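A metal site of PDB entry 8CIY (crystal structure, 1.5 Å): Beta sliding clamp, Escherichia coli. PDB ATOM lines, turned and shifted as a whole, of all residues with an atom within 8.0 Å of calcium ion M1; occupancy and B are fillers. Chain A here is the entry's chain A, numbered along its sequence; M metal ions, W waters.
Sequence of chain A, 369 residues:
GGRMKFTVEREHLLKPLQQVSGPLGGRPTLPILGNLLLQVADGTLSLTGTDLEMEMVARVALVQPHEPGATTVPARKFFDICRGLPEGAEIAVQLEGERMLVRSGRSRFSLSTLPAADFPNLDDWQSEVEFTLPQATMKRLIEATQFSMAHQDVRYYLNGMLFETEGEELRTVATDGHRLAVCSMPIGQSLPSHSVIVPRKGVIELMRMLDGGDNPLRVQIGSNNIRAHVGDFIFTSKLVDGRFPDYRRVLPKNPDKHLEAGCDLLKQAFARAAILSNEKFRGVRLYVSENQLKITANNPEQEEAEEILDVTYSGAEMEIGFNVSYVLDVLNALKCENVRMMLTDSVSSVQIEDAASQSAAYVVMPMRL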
ATOM      1  N   VAL A   8       1.702   4.870  22.505  1.00  0.00           N
ATOM      2  CA  VAL A   8       2.043   4.874  23.926  1.00  0.00           C
ATOM      3  C   VAL A   8       3.241   3.972  24.181  1.00  0.00           C
ATOM      4  O   VAL A   8       3.382   2.919  23.569  1.00  0.00           O
ATOM      5  CB  VAL A   8       0.813   4.462  24.763  1.00  0.00           C
ATOM      6  CG1 VAL A   8       0.391   3.030  24.452  1.00  0.00           C
ATOM      7  CG2 VAL A   8       1.067   4.634  26.267  1.00  0.00           C
ATOM      8  N   GLU A   9       4.093   4.386  25.118  1.00  0.00           N
ATOM      9  CA  GLU A   9       5.197   3.537  25.539  1.00  0.00           C
ATOM     10  C   GLU A   9       4.667   2.284  26.214  1.00  0.00           C
ATOM     11  O   GLU A   9       3.783   2.339  27.063  1.00  0.00           O
ATOM     12  CB  GLU A   9       6.102   4.280  26.519  1.00  0.00           C
ATOM     13  CG  GLU A   9       6.933   5.364  25.857  1.00  0.00           C
ATOM     14  CD  GLU A   9       8.160   4.833  25.151  1.00  0.00           C
ATOM     15  OE1 GLU A   9       8.468   3.624  25.323  1.00  0.00           O
ATOM     16  OE2 GLU A   9       8.834   5.607  24.450  1.00  0.00           O
ATOM     17  N   ARG A  10       5.290   1.150  25.882  1.00  0.00           N
ATOM     18  CA  ARG A  10       4.971  -0.117  26.529  1.00  0.00           C
ATOM     19  C   ARG A  10       4.895   0.026  28.049  1.00  0.00           C
ATOM     20  O   ARG A  10       3.936  -0.439  28.685  1.00  0.00           O
ATOM     21  CB  ARG A  10       6.025  -1.156  26.157  1.00  0.00           C
ATOM     22  CG  ARG A  10       5.854  -2.502  26.844  1.00  0.00           C
ATOM     23  CD  ARG A  10       6.880  -3.482  26.311  1.00  0.00           C
ATOM     24  NE  ARG A  10       6.836  -4.778  26.970  1.00  0.00           N
ATOM     25  CZ  ARG A  10       7.451  -5.053  28.103  1.00  0.00           C
ATOM     26  NH1 ARG A  10       8.155  -4.137  28.754  1.00  0.00           N
ATOM     27  NH2 ARG A  10       7.384  -6.299  28.598  1.00  0.00           N
ATOM     28  N   GLU A  11       5.917   0.618  28.654  1.00  0.00           N
ATOM     29  CA  GLU A  11       5.944   0.613  30.112  1.00  0.00           C
ATOM     30  C   GLU A  11       4.923   1.567  30.731  1.00  0.00           C
ATOM     31  O   GLU A  11       4.667   1.455  31.920  1.00  0.00           O
ATOM     32  CB  GLU A  11       7.383   0.866  30.563  1.00  0.00           C
ATOM     33  CG  GLU A  11       8.203  -0.465  30.465  1.00  0.00           C
ATOM     34  CD  GLU A  11       9.066  -0.523  29.217  1.00  0.00           C
ATOM     35  OE1 GLU A  11       9.936   0.351  29.066  1.00  0.00           O
ATOM     36  OE2 GLU A  11       8.872  -1.395  28.359  1.00  0.00           O
ATOM     37  N   PRO A  86       9.368  -5.859  23.046  1.00  0.00           N
ATOM     38  CA  PRO A  86      10.622  -5.595  23.761  1.00  0.00           C
ATOM     39  C   PRO A  86      10.503  -4.407  24.705  1.00  0.00           C
ATOM     40  O   PRO A  86       9.690  -3.502  24.522  1.00  0.00           O
ATOM     41  CB  PRO A  86      11.623  -5.320  22.637  1.00  0.00           C
ATOM     42  CG  PRO A  86      10.821  -4.875  21.495  1.00  0.00           C
ATOM     43  CD  PRO A  86       9.522  -5.637  21.605  1.00  0.00           C
ATOM     44  N   GLU A  87      11.362  -4.429  25.743  1.00  0.00           N
ATOM     45  CA  GLU A  87      11.397  -3.326  26.682  1.00  0.00           C
ATOM     46  C   GLU A  87      11.641  -2.026  25.916  1.00  0.00           C
ATOM     47  O   GLU A  87      12.510  -1.964  25.046  1.00  0.00           O
ATOM     48  CB  GLU A  87      12.503  -3.541  27.711  1.00  0.00           C
ATOM     49  CG  GLU A  87      12.413  -2.591  28.907  1.00  0.00           C
ATOM     50  CD  GLU A  87      13.311  -3.011  30.051  1.00  0.00           C
ATOM     51  OE1 GLU A  87      13.895  -4.111  29.999  1.00  0.00           O
ATOM     52  OE2 GLU A  87      13.415  -2.229  31.031  1.00  0.00           O
ATOM     53  N   GLY A  88      10.863  -0.995  26.244  1.00  0.00           N
ATOM     54  CA  GLY A  88      11.021   0.300  25.633  1.00  0.00           C
ATOM     55  C   GLY A  88      10.204   0.492  24.362  1.00  0.00           C
ATOM     56  O   GLY A  88      10.226   1.590  23.787  1.00  0.00           O
ATOM     57  N   ALA A  89       9.495  -0.527  23.917  1.00  0.00           N
ATOM     58  CA  ALA A  89       8.768  -0.427  22.658  1.00  0.00           C
ATOM     59  C   ALA A  89       7.699   0.670  22.709  1.00  0.00           C
ATOM     60  O   ALA A  89       7.046   0.874  23.733  1.00  0.00           O
ATOM     61  CB  ALA A  89       8.127  -1.773  22.349  1.00  0.00           C
ATOM     62  N   GLU A  90       7.523   1.357  21.582  1.00  0.00           N
ATOM     63  CA  GLU A  90       6.381   2.244  21.388  1.00  0.00           C
ATOM     64  C   GLU A  90       5.302   1.471  20.657  1.00  0.00           C
ATOM     65  O   GLU A  90       5.581   0.747  19.706  1.00  0.00           O
ATOM     66  CB  GLU A  90       6.767   3.484  20.595  1.00  0.00           C
ATOM     67  CG  GLU A  90       7.835   4.342  21.250  1.00  0.00           C
ATOM     68  CD  GLU A  90       9.234   3.946  20.851  1.00  0.00           C
ATOM     69  OE1 GLU A  90       9.437   3.604  19.667  1.00  0.00           O
ATOM     70  OE2 GLU A  90      10.148   3.979  21.709  1.00  0.00           O
ATOM     71  N   ILE A  91       4.065   1.614  21.127  1.00  0.00           N
ATOM     72  CA  ILE A  91       2.941   0.822  20.655  1.00  0.00           C
ATOM     73  C   ILE A  91       1.934   1.769  20.030  1.00  0.00           C
ATOM     74  O   ILE A  91       1.379   2.636  20.712  1.00  0.00           O
ATOM     75  CB  ILE A  91       2.320   0.018  21.809  1.00  0.00           C
ATOM     76  CG1 ILE A  91       3.391  -0.873  22.427  1.00  0.00           C
ATOM     77  CG2 ILE A  91       1.134  -0.817  21.306  1.00  0.00           C
ATOM     78  CD1 ILE A  91       2.956  -1.610  23.647  1.00  0.00           C
HETATM   79 CA    CA M   1      10.614   3.889  24.021  1.00  0.00          CA
HETATM   80 CA    CA M   2      11.518   1.469  29.995  1.00  0.00          CA
HETATM   81  O   HOH W   1      12.795   3.053  23.596  1.00  0.00           O
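The backbone NH (N) of Gly 88 sits at hydrogen-bond distance from the side-chain carboxylate (OE2) of Glu 11 (2.9 Å).
Within 4 Å of calcium ion M1: Glu 9, Gly 88 and Glu 90.
The nearest printed residue that does not touch calcium ion M1 is Ala 89 (4.5 Å).
Calcium ion M1 is bound by O of Gly 88, OE2 of Glu 90, water W1, OE2 of Glu 9 and OE1 of Glu 9.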
